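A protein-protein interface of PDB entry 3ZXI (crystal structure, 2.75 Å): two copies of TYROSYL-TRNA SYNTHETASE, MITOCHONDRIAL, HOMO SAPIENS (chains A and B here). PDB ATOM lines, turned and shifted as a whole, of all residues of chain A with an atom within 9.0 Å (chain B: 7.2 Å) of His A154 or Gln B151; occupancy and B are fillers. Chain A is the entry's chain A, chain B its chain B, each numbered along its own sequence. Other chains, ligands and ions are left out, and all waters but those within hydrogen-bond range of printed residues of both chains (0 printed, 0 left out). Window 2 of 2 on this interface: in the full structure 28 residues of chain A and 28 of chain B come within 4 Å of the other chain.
The backbone carbonyl oxygen (O) of Gln A153 lies within hydrogen-bond range of the backbone NH (N) of Leu B155 (2.9 Å).
A ring nitrogen (NE2) of His B154 is in hydrogen-bond range of a ring nitrogen (NE2) of His A154, at 2.8 Å.
N of Leu B155 lies close to N of Leu A155.
OD1 of Asp A157 lies within salt-bridge range of NH1 of Arg B91 (2.8 Å).
The backbone NH (N) of Leu A155 sits at hydrogen-bond distance from the backbone carbonyl oxygen (O) of Gln B153, 3.1 Å away.
OD1 of Asn B146 sits at hydrogen-bond distance from N of Ala B88 (3.1 Å).
The side-chain amide oxygen (OE1) of Gln B151 sits close to the backbone carbonyl oxygen (O) of Ser B147 (3.5 Å).
CD2 of His B154 touches O of Gln A151, at 3.6 Å.
His B154 touches Gln A153 (CA to O, 3.4 Å).
Gln B151 touches His A154.
CA of His A154 touches O of Gln B153 (3.3 Å).
Leu B155 touches His A154.
CG1 of Val A156 touches O of Ala B88 (3.6 Å).
Val A156 touches Arg B91.
Phe A158 touches Leu B155 (CG to CD1, 3.3 Å).
Ala A160 touches Arg B91.
Of the printed residues of chain B, His A154 touches Gln B151 (3.6 Å), Gln B153 (3.3 Å), His B154 (2.8 Å) and Leu B155 (3.99 Å).
Printed residues of chain B within 4 Å of Asp A157: Arg B91.
Of the printed residues of chain B, Phe A158 touches Leu B155 (3.3 Å).
Of the printed residues of chain A, Gln B151 touches His A154.
Of the printed residues of chain A, Gln B153 touches His A154 (3.3 Å) and Leu A155 (3.1 Å).
The nearest printed residue of chain B that does not touch His A154 is Lys B152 (4.4 Å).
The nearest printed residue of chain A that does not touch His B154 is Leu A155 (4.1 Å).
Of the 14 printed residues of chain A, 8 touch a printed residue of chain B.
Printed residues of chain A that touch a printed residue of chain B: Gln A151, Gln A153, His A154, Leu A155, Val A156, Asp A157, Phe A158 and Ala A160.
Hydrophobic or aromatic side chains of chain A that line the printed part of chain B: His A154, Leu A155, Val A156, Phe A158 and Ala A160.
Among the printed residues, 14 pairs touch across the chains.
Among the printed residues, Asp or Glu carboxylates within 4 Å of a Lys or Arg side-chain nitrogen of the other chain: Asp A157 with Arg B91 (2.8 Å).
Gln A153 touches His B154, and with the chains exchanged His A154 touches Gln B153.
Gln A153 touches Leu B155, and with the chains exchanged Leu A155 touches Gln B153.
His A154 touches its own counterpart, His B154.
His A154 touches Leu B155, but with the chains exchanged Leu A155 does not touch His B154 (4.1 Å).
Positions printed for both chains: 149, 150, 151, 152, 153, 154, 155 and 156.
Of the 14 pairs that touch across the chains among the printed residues, 8 have their exchanged pair printed and touching as well.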
ATOM      1  N   TRP A 149     -11.659 -41.958  19.678  1.00  0.00           N
ATOM      2  CA  TRP A 149     -10.612 -40.942  19.527  1.00  0.00           C
ATOM      3  C   TRP A 149     -10.931 -39.590  20.163  1.00  0.00           C
ATOM      4  O   TRP A 149     -10.027 -38.770  20.341  1.00  0.00           O
ATOM      5  CB  TRP A 149     -10.156 -40.759  18.072  1.00  0.00           C
ATOM      6  CG  TRP A 149     -11.220 -40.371  17.084  1.00  0.00           C
ATOM      7  CD1 TRP A 149     -11.651 -39.107  16.781  1.00  0.00           C
ATOM      8  CD2 TRP A 149     -11.959 -41.255  16.243  1.00  0.00           C
ATOM      9  NE1 TRP A 149     -12.626 -39.159  15.828  1.00  0.00           N
ATOM     10  CE2 TRP A 149     -12.834 -40.466  15.478  1.00  0.00           C
ATOM     11  CE3 TRP A 149     -11.977 -42.646  16.073  1.00  0.00           C
ATOM     12  CZ2 TRP A 149     -13.703 -41.020  14.539  1.00  0.00           C
ATOM     13  CZ3 TRP A 149     -12.849 -43.191  15.154  1.00  0.00           C
ATOM     14  CH2 TRP A 149     -13.697 -42.383  14.396  1.00  0.00           C
ATOM     15  N   TYR A 150     -12.202 -39.360  20.495  1.00  0.00           N
ATOM     16  CA  TYR A 150     -12.599 -38.128  21.191  1.00  0.00           C
ATOM     17  C   TYR A 150     -12.347 -38.179  22.707  1.00  0.00           C
ATOM     18  O   TYR A 150     -12.035 -37.163  23.326  1.00  0.00           O
ATOM     19  CB  TYR A 150     -14.041 -37.724  20.826  1.00  0.00           C
ATOM     20  CG  TYR A 150     -14.086 -37.015  19.469  1.00  0.00           C
ATOM     21  CD1 TYR A 150     -13.091 -36.091  19.123  1.00  0.00           C
ATOM     22  CD2 TYR A 150     -15.084 -37.295  18.521  1.00  0.00           C
ATOM     23  CE1 TYR A 150     -13.096 -35.443  17.900  1.00  0.00           C
ATOM     24  CE2 TYR A 150     -15.092 -36.654  17.287  1.00  0.00           C
ATOM     25  CZ  TYR A 150     -14.096 -35.727  16.986  1.00  0.00           C
ATOM     26  OH  TYR A 150     -14.086 -35.081  15.780  1.00  0.00           O
ATOM     27  N   GLN A 151     -12.447 -39.377  23.275  1.00  0.00           N
ATOM     28  CA  GLN A 151     -12.110 -39.617  24.661  1.00  0.00           C
ATOM     29  C   GLN A 151     -10.640 -39.330  25.010  1.00  0.00           C
ATOM     30  O   GLN A 151     -10.274 -39.294  26.186  1.00  0.00           O
ATOM     31  CB  GLN A 151     -12.487 -41.048  25.059  1.00  0.00           C
ATOM     32  CG  GLN A 151     -13.918 -41.167  25.559  1.00  0.00           C
ATOM     33  CD  GLN A 151     -14.476 -42.559  25.433  1.00  0.00           C
ATOM     34  OE1 GLN A 151     -13.754 -43.503  25.106  1.00  0.00           O
ATOM     35  NE2 GLN A 151     -15.778 -42.696  25.679  1.00  0.00           N
ATOM     36  N   LYS A 152      -9.803 -39.112  24.005  1.00  0.00           N
ATOM     37  CA  LYS A 152      -8.403 -38.801  24.263  1.00  0.00           C
ATOM     38  C   LYS A 152      -8.115 -37.356  23.852  1.00  0.00           C
ATOM     39  O   LYS A 152      -6.961 -36.919  23.827  1.00  0.00           O
ATOM     40  CB  LYS A 152      -7.472 -39.770  23.510  1.00  0.00           C
ATOM     41  CG  LYS A 152      -7.942 -41.223  23.479  1.00  0.00           C
ATOM     42  CD  LYS A 152      -7.682 -41.964  24.789  1.00  0.00           C
ATOM     43  CE  LYS A 152      -6.225 -42.436  24.887  1.00  0.00           C
ATOM     44  NZ  LYS A 152      -6.069 -43.692  25.680  1.00  0.00           N
ATOM     45  N   GLN A 153      -9.173 -36.614  23.543  1.00  0.00           N
ATOM     46  CA  GLN A 153      -9.026 -35.257  23.022  1.00  0.00           C
ATOM     47  C   GLN A 153      -9.397 -34.154  24.007  1.00  0.00           C
ATOM     48  O   GLN A 153     -10.567 -33.982  24.342  1.00  0.00           O
ATOM     49  CB  GLN A 153      -9.855 -35.093  21.743  1.00  0.00           C
ATOM     50  CG  GLN A 153      -9.055 -35.226  20.462  1.00  0.00           C
ATOM     51  CD  GLN A 153      -7.982 -34.165  20.335  1.00  0.00           C
ATOM     52  OE1 GLN A 153      -7.110 -34.245  19.473  1.00  0.00           O
ATOM     53  NE2 GLN A 153      -8.042 -33.165  21.196  1.00  0.00           N
ATOM     54  N   HIS A 154      -8.395 -33.388  24.435  1.00  0.00           N
ATOM     55  CA  HIS A 154      -8.625 -32.250  25.333  1.00  0.00           C
ATOM     56  C   HIS A 154      -8.884 -30.938  24.590  1.00  0.00           C
ATOM     57  O   HIS A 154      -8.121 -30.552  23.700  1.00  0.00           O
ATOM     58  CB  HIS A 154      -7.459 -32.073  26.308  1.00  0.00           C
ATOM     59  CG  HIS A 154      -7.323 -33.191  27.293  1.00  0.00           C
ATOM     60  ND1 HIS A 154      -6.370 -34.181  27.171  1.00  0.00           N
ATOM     61  CD2 HIS A 154      -8.028 -33.484  28.413  1.00  0.00           C
ATOM     62  CE1 HIS A 154      -6.497 -35.034  28.169  1.00  0.00           C
ATOM     63  NE2 HIS A 154      -7.494 -34.635  28.937  1.00  0.00           N
ATOM     64  N   LEU A 155      -9.965 -30.272  24.993  1.00  0.00           N
ATOM     65  CA  LEU A 155     -10.424 -29.000  24.437  1.00  0.00           C
ATOM     66  C   LEU A 155      -9.331 -28.114  23.834  1.00  0.00           C
ATOM     67  O   LEU A 155      -9.249 -27.975  22.606  1.00  0.00           O
ATOM     68  CB  LEU A 155     -11.196 -28.216  25.501  1.00  0.00           C
ATOM     69  CG  LEU A 155     -11.796 -26.916  24.995  1.00  0.00           C
ATOM     70  CD1 LEU A 155     -13.291 -26.947  25.118  1.00  0.00           C
ATOM     71  CD2 LEU A 155     -11.239 -25.793  25.799  1.00  0.00           C
ATOM     72  N   VAL A 156      -8.498 -27.520  24.687  1.00  0.00           N
ATOM     73  CA  VAL A 156      -7.493 -26.553  24.213  1.00  0.00           C
ATOM     74  C   VAL A 156      -6.472 -27.192  23.255  1.00  0.00           C
ATOM     75  O   VAL A 156      -5.926 -26.537  22.369  1.00  0.00           O
ATOM     76  CB  VAL A 156      -6.778 -25.780  25.376  1.00  0.00           C
ATOM     77  CG1 VAL A 156      -5.752 -24.794  24.831  1.00  0.00           C
ATOM     78  CG2 VAL A 156      -7.785 -25.016  26.194  1.00  0.00           C
ATOM     79  N   ASP A 157      -6.219 -28.479  23.413  1.00  0.00           N
ATOM     80  CA  ASP A 157      -5.290 -29.142  22.501  1.00  0.00           C
ATOM     81  C   ASP A 157      -5.875 -29.193  21.098  1.00  0.00           C
ATOM     82  O   ASP A 157      -5.261 -28.742  20.117  1.00  0.00           O
ATOM     83  CB  ASP A 157      -4.975 -30.545  23.005  1.00  0.00           C
ATOM     84  CG  ASP A 157      -4.261 -30.528  24.341  1.00  0.00           C
ATOM     85  OD1 ASP A 157      -3.102 -30.059  24.382  1.00  0.00           O
ATOM     86  OD2 ASP A 157      -4.856 -30.975  25.345  1.00  0.00           O
ATOM     87  N   PHE A 158      -7.074 -29.749  21.011  1.00  0.00           N
ATOM     88  CA  PHE A 158      -7.827 -29.710  19.759  1.00  0.00           C
ATOM     89  C   PHE A 158      -7.811 -28.305  19.166  1.00  0.00           C
ATOM     90  O   PHE A 158      -7.324 -28.113  18.066  1.00  0.00           O
ATOM     91  CB  PHE A 158      -9.267 -30.122  20.027  1.00  0.00           C
ATOM     92  CG  PHE A 158     -10.091 -30.286  18.796  1.00  0.00           C
ATOM     93  CD1 PHE A 158     -10.364 -29.206  17.982  1.00  0.00           C
ATOM     94  CD2 PHE A 158     -10.625 -31.530  18.470  1.00  0.00           C
ATOM     95  CE1 PHE A 158     -11.139 -29.359  16.843  1.00  0.00           C
ATOM     96  CE2 PHE A 158     -11.400 -31.696  17.336  1.00  0.00           C
ATOM     97  CZ  PHE A 158     -11.657 -30.607  16.515  1.00  0.00           C
ATOM     98  N   LEU A 159      -8.343 -27.336  19.914  1.00  0.00           N
ATOM     99  CA  LEU A 159      -8.425 -25.960  19.462  1.00  0.00           C
ATOM    100  C   LEU A 159      -7.061 -25.466  19.022  1.00  0.00           C
ATOM    101  O   LEU A 159      -6.918 -24.753  18.010  1.00  0.00           O
ATOM    102  CB  LEU A 159      -8.954 -25.066  20.574  1.00  0.00           C
ATOM    103  CG  LEU A 159     -10.419 -25.305  20.883  1.00  0.00           C
ATOM    104  CD1 LEU A 159     -10.849 -24.361  21.983  1.00  0.00           C
ATOM    105  CD2 LEU A 159     -11.209 -25.068  19.605  1.00  0.00           C
ATOM    106  N   ALA A 160      -6.049 -25.856  19.782  1.00  0.00           N
ATOM    107  CA  ALA A 160      -4.701 -25.382  19.514  1.00  0.00           C
ATOM    108  C   ALA A 160      -4.168 -26.013  18.254  1.00  0.00           C
ATOM    109  O   ALA A 160      -3.430 -25.386  17.503  1.00  0.00           O
ATOM    110  CB  ALA A 160      -3.786 -25.695  20.671  1.00  0.00           C
ATOM    111  N   ALA A 161      -4.547 -27.265  18.033  1.00  0.00           N
ATOM    112  CA  ALA A 161      -3.995 -28.047  16.934  1.00  0.00           C
ATOM    113  C   ALA A 161      -4.663 -27.749  15.593  1.00  0.00           C
ATOM    114  O   ALA A 161      -4.001 -27.707  14.556  1.00  0.00           O
ATOM    115  CB  ALA A 161      -4.104 -29.516  17.254  1.00  0.00           C
ATOM    116  N   VAL A 162      -5.972 -27.532  15.622  1.00  0.00           N
ATOM    117  CA  VAL A 162      -6.751 -27.466  14.391  1.00  0.00           C
ATOM    118  C   VAL A 162      -7.554 -26.169  14.247  1.00  0.00           C
ATOM    119  O   VAL A 162      -7.692 -25.647  13.144  1.00  0.00           O
ATOM    120  CB  VAL A 162      -7.712 -28.670  14.301  1.00  0.00           C
ATOM    121  CG1 VAL A 162      -7.153 -29.838  15.103  1.00  0.00           C
ATOM    122  CG2 VAL A 162      -9.083 -28.299  14.843  1.00  0.00           C
ATOM    123  N   ALA B  88      -3.182 -22.236  29.433  1.00  0.00           N
ATOM    124  CA  ALA B  88      -4.023 -22.731  28.341  1.00  0.00           C
ATOM    125  C   ALA B  88      -4.280 -21.706  27.221  1.00  0.00           C
ATOM    126  O   ALA B  88      -3.979 -21.960  26.051  1.00  0.00           O
ATOM    127  CB  ALA B  88      -5.351 -23.240  28.897  1.00  0.00           C
ATOM    128  N   ARG B  91      -1.879 -20.500  24.292  1.00  0.00           N
ATOM    129  CA  ARG B  91      -1.603 -21.439  23.220  1.00  0.00           C
ATOM    130  C   ARG B  91      -2.404 -21.030  21.998  1.00  0.00           C
ATOM    131  O   ARG B  91      -1.931 -21.112  20.863  1.00  0.00           O
ATOM    132  CB  ARG B  91      -2.005 -22.840  23.660  1.00  0.00           C
ATOM    133  CG  ARG B  91      -1.443 -23.230  25.035  1.00  0.00           C
ATOM    134  CD  ARG B  91      -1.807 -24.669  25.373  1.00  0.00           C
ATOM    135  NE  ARG B  91      -1.449 -25.580  24.283  1.00  0.00           N
ATOM    136  CZ  ARG B  91      -1.898 -26.826  24.177  1.00  0.00           C
ATOM    137  NH1 ARG B  91      -2.734 -27.323  25.090  1.00  0.00           N
ATOM    138  NH2 ARG B  91      -1.502 -27.575  23.159  1.00  0.00           N
ATOM    139  N   ARG B 111       4.547 -23.089  27.929  1.00  0.00           N
ATOM    140  CA  ARG B 111       4.679 -23.679  29.259  1.00  0.00           C
ATOM    141  C   ARG B 111       5.793 -22.997  30.038  1.00  0.00           C
ATOM    142  O   ARG B 111       5.693 -22.822  31.254  1.00  0.00           O
ATOM    143  CB  ARG B 111       4.960 -25.188  29.160  1.00  0.00           C
ATOM    144  CG  ARG B 111       3.810 -26.029  28.554  1.00  0.00           C
ATOM    145  CD  ARG B 111       2.726 -26.350  29.597  1.00  0.00           C
ATOM    146  NE  ARG B 111       1.578 -27.093  29.055  1.00  0.00           N
ATOM    147  CZ  ARG B 111       0.451 -26.530  28.615  1.00  0.00           C
ATOM    148  NH1 ARG B 111       0.305 -25.212  28.635  1.00  0.00           N
ATOM    149  NH2 ARG B 111      -0.538 -27.281  28.155  1.00  0.00           N
ATOM    150  N   ASP B 145      -3.314 -20.606  37.639  1.00  0.00           N
ATOM    151  CA  ASP B 145      -3.113 -20.903  36.224  1.00  0.00           C
ATOM    152  C   ASP B 145      -4.313 -21.701  35.711  1.00  0.00           C
ATOM    153  O   ASP B 145      -4.723 -22.665  36.359  1.00  0.00           O
ATOM    154  CB  ASP B 145      -1.823 -21.697  36.037  1.00  0.00           C
ATOM    155  CG  ASP B 145      -1.506 -21.969  34.582  1.00  0.00           C
ATOM    156  OD1 ASP B 145      -2.448 -22.072  33.774  1.00  0.00           O
ATOM    157  OD2 ASP B 145      -0.310 -22.077  34.242  1.00  0.00           O
ATOM    158  N   ASN B 146      -4.881 -21.303  34.568  1.00  0.00           N
ATOM    159  CA  ASN B 146      -6.019 -22.039  33.969  1.00  0.00           C
ATOM    160  C   ASN B 146      -5.692 -23.405  33.320  1.00  0.00           C
ATOM    161  O   ASN B 146      -6.582 -24.232  33.106  1.00  0.00           O
ATOM    162  CB  ASN B 146      -6.833 -21.157  32.999  1.00  0.00           C
ATOM    163  CG  ASN B 146      -5.971 -20.432  31.974  1.00  0.00           C
ATOM    164  OD1 ASN B 146      -4.831 -20.821  31.698  1.00  0.00           O
ATOM    165  ND2 ASN B 146      -6.522 -19.365  31.402  1.00  0.00           N
ATOM    166  N   SER B 147      -4.422 -23.634  33.007  1.00  0.00           N
ATOM    167  CA  SER B 147      -3.989 -24.933  32.520  1.00  0.00           C
ATOM    168  C   SER B 147      -4.307 -26.005  33.554  1.00  0.00           C
ATOM    169  O   SER B 147      -4.659 -27.117  33.216  1.00  0.00           O
ATOM    170  CB  SER B 147      -2.511 -24.933  32.156  1.00  0.00           C
ATOM    171  OG  SER B 147      -1.699 -24.739  33.288  1.00  0.00           O
ATOM    172  N   ALA B 148      -4.233 -25.642  34.819  1.00  0.00           N
ATOM    173  CA  ALA B 148      -4.627 -26.538  35.889  1.00  0.00           C
ATOM    174  C   ALA B 148      -5.988 -27.173  35.672  1.00  0.00           C
ATOM    175  O   ALA B 148      -6.160 -28.361  35.948  1.00  0.00           O
ATOM    176  CB  ALA B 148      -4.607 -25.813  37.216  1.00  0.00           C
ATOM    177  N   TRP B 149      -6.970 -26.392  35.229  1.00  0.00           N
ATOM    178  CA  TRP B 149      -8.318 -26.938  35.046  1.00  0.00           C
ATOM    179  C   TRP B 149      -8.643 -27.334  33.617  1.00  0.00           C
ATOM    180  O   TRP B 149      -9.572 -28.144  33.383  1.00  0.00           O
ATOM    181  CB  TRP B 149      -9.424 -26.051  35.636  1.00  0.00           C
ATOM    182  CG  TRP B 149      -9.505 -24.632  35.137  1.00  0.00           C
ATOM    183  CD1 TRP B 149     -10.192 -24.183  34.050  1.00  0.00           C
ATOM    184  CD2 TRP B 149      -8.915 -23.470  35.743  1.00  0.00           C
ATOM    185  NE1 TRP B 149     -10.047 -22.822  33.926  1.00  0.00           N
ATOM    186  CE2 TRP B 149      -9.266 -22.364  34.952  1.00  0.00           C
ATOM    187  CE3 TRP B 149      -8.116 -23.265  36.868  1.00  0.00           C
ATOM    188  CZ2 TRP B 149      -8.857 -21.078  35.254  1.00  0.00           C
ATOM    189  CZ3 TRP B 149      -7.711 -21.992  37.157  1.00  0.00           C
ATOM    190  CH2 TRP B 149      -8.077 -20.915  36.355  1.00  0.00           C
ATOM    191  N   TYR B 150      -7.880 -26.782  32.670  1.00  0.00           N
ATOM    192  CA  TYR B 150      -8.031 -27.175  31.262  1.00  0.00           C
ATOM    193  C   TYR B 150      -7.411 -28.551  30.930  1.00  0.00           C
ATOM    194  O   TYR B 150      -7.940 -29.295  30.095  1.00  0.00           O
ATOM    195  CB  TYR B 150      -7.601 -26.043  30.293  1.00  0.00           C
ATOM    196  CG  TYR B 150      -8.683 -24.979  30.176  1.00  0.00           C
ATOM    197  CD1 TYR B 150     -10.030 -25.342  30.101  1.00  0.00           C
ATOM    198  CD2 TYR B 150      -8.374 -23.613  30.201  1.00  0.00           C
ATOM    199  CE1 TYR B 150     -11.038 -24.376  30.027  1.00  0.00           C
ATOM    200  CE2 TYR B 150      -9.376 -22.652  30.130  1.00  0.00           C
ATOM    201  CZ  TYR B 150     -10.705 -23.034  30.037  1.00  0.00           C
ATOM    202  OH  TYR B 150     -11.695 -22.065  29.968  1.00  0.00           O
ATOM    203  N   GLN B 151      -6.320 -28.894  31.611  1.00  0.00           N
ATOM    204  CA  GLN B 151      -5.698 -30.207  31.460  1.00  0.00           C
ATOM    205  C   GLN B 151      -6.598 -31.367  31.892  1.00  0.00           C
ATOM    206  O   GLN B 151      -6.277 -32.523  31.633  1.00  0.00           O
ATOM    207  CB  GLN B 151      -4.379 -30.269  32.226  1.00  0.00           C
ATOM    208  CG  GLN B 151      -3.171 -29.832  31.415  1.00  0.00           C
ATOM    209  CD  GLN B 151      -2.038 -29.280  32.280  1.00  0.00           C
ATOM    210  OE1 GLN B 151      -2.066 -29.388  33.515  1.00  0.00           O
ATOM    211  NE2 GLN B 151      -1.040 -28.671  31.632  1.00  0.00           N
ATOM    212  N   LYS B 152      -7.716 -31.075  32.549  1.00  0.00           N
ATOM    213  CA  LYS B 152      -8.646 -32.141  32.923  1.00  0.00           C
ATOM    214  C   LYS B 152      -9.919 -32.056  32.104  1.00  0.00           C
ATOM    215  O   LYS B 152     -10.898 -32.737  32.410  1.00  0.00           O
ATOM    216  CB  LYS B 152      -8.997 -32.077  34.410  1.00  0.00           C
ATOM    217  CG  LYS B 152      -7.829 -31.705  35.308  1.00  0.00           C
ATOM    218  CD  LYS B 152      -6.873 -32.860  35.590  1.00  0.00           C
ATOM    219  CE  LYS B 152      -7.417 -33.761  36.691  1.00  0.00           C
ATOM    220  NZ  LYS B 152      -6.328 -34.405  37.482  1.00  0.00           N
ATOM    221  N   GLN B 153      -9.898 -31.212  31.068  1.00  0.00           N
ATOM    222  CA  GLN B 153     -11.085 -30.916  30.248  1.00  0.00           C
ATOM    223  C   GLN B 153     -11.083 -31.515  28.827  1.00  0.00           C
ATOM    224  O   GLN B 153     -10.340 -31.066  27.951  1.00  0.00           O
ATOM    225  CB  GLN B 153     -11.302 -29.408  30.161  1.00  0.00           C
ATOM    226  CG  GLN B 153     -12.337 -28.886  31.132  1.00  0.00           C
ATOM    227  CD  GLN B 153     -13.716 -29.465  30.891  1.00  0.00           C
ATOM    228  OE1 GLN B 153     -14.640 -29.245  31.673  1.00  0.00           O
ATOM    229  NE2 GLN B 153     -13.869 -30.203  29.794  1.00  0.00           N
ATOM    230  N   HIS B 154     -11.930 -32.519  28.606  1.00  0.00           N
ATOM    231  CA  HIS B 154     -12.054 -33.149  27.289  1.00  0.00           C
ATOM    232  C   HIS B 154     -13.087 -32.461  26.382  1.00  0.00           C
ATOM    233  O   HIS B 154     -14.246 -32.238  26.770  1.00  0.00           O
ATOM    234  CB  HIS B 154     -12.390 -34.644  27.417  1.00  0.00           C
ATOM    235  CG  HIS B 154     -11.289 -35.466  28.019  1.00  0.00           C
ATOM    236  ND1 HIS B 154     -11.311 -35.898  29.329  1.00  0.00           N
ATOM    237  CD2 HIS B 154     -10.129 -35.927  27.491  1.00  0.00           C
ATOM    238  CE1 HIS B 154     -10.214 -36.586  29.581  1.00  0.00           C
ATOM    239  NE2 HIS B 154      -9.477 -36.615  28.484  1.00  0.00           N
ATOM    240  N   LEU B 155     -12.639 -32.152  25.167  1.00  0.00           N
ATOM    241  CA  LEU B 155     -13.435 -31.502  24.133  1.00  0.00           C
ATOM    242  C   LEU B 155     -14.958 -31.711  24.191  1.00  0.00           C
ATOM    243  O   LEU B 155     -15.686 -30.773  24.558  1.00  0.00           O
ATOM    244  CB  LEU B 155     -12.915 -31.899  22.760  1.00  0.00           C
ATOM    245  CG  LEU B 155     -13.647 -31.194  21.620  1.00  0.00           C
ATOM    246  CD1 LEU B 155     -12.700 -30.356  20.804  1.00  0.00           C
ATOM    247  CD2 LEU B 155     -14.306 -32.226  20.754  1.00  0.00           C
ATOM    248  N   VAL B 156     -15.432 -32.907  23.808  1.00  0.00           N
ATOM    249  CA  VAL B 156     -16.867 -33.201  23.798  1.00  0.00           C
ATOM    250  C   VAL B 156     -17.553 -33.057  25.164  1.00  0.00           C
ATOM    251  O   VAL B 156     -18.740 -32.727  25.236  1.00  0.00           O
ATOM    252  CB  VAL B 156     -17.200 -34.579  23.144  1.00  0.00           C
ATOM    253  CG1 VAL B 156     -18.721 -34.824  23.063  1.00  0.00           C
ATOM    254  CG2 VAL B 156     -16.634 -34.653  21.760  1.00  0.00           C
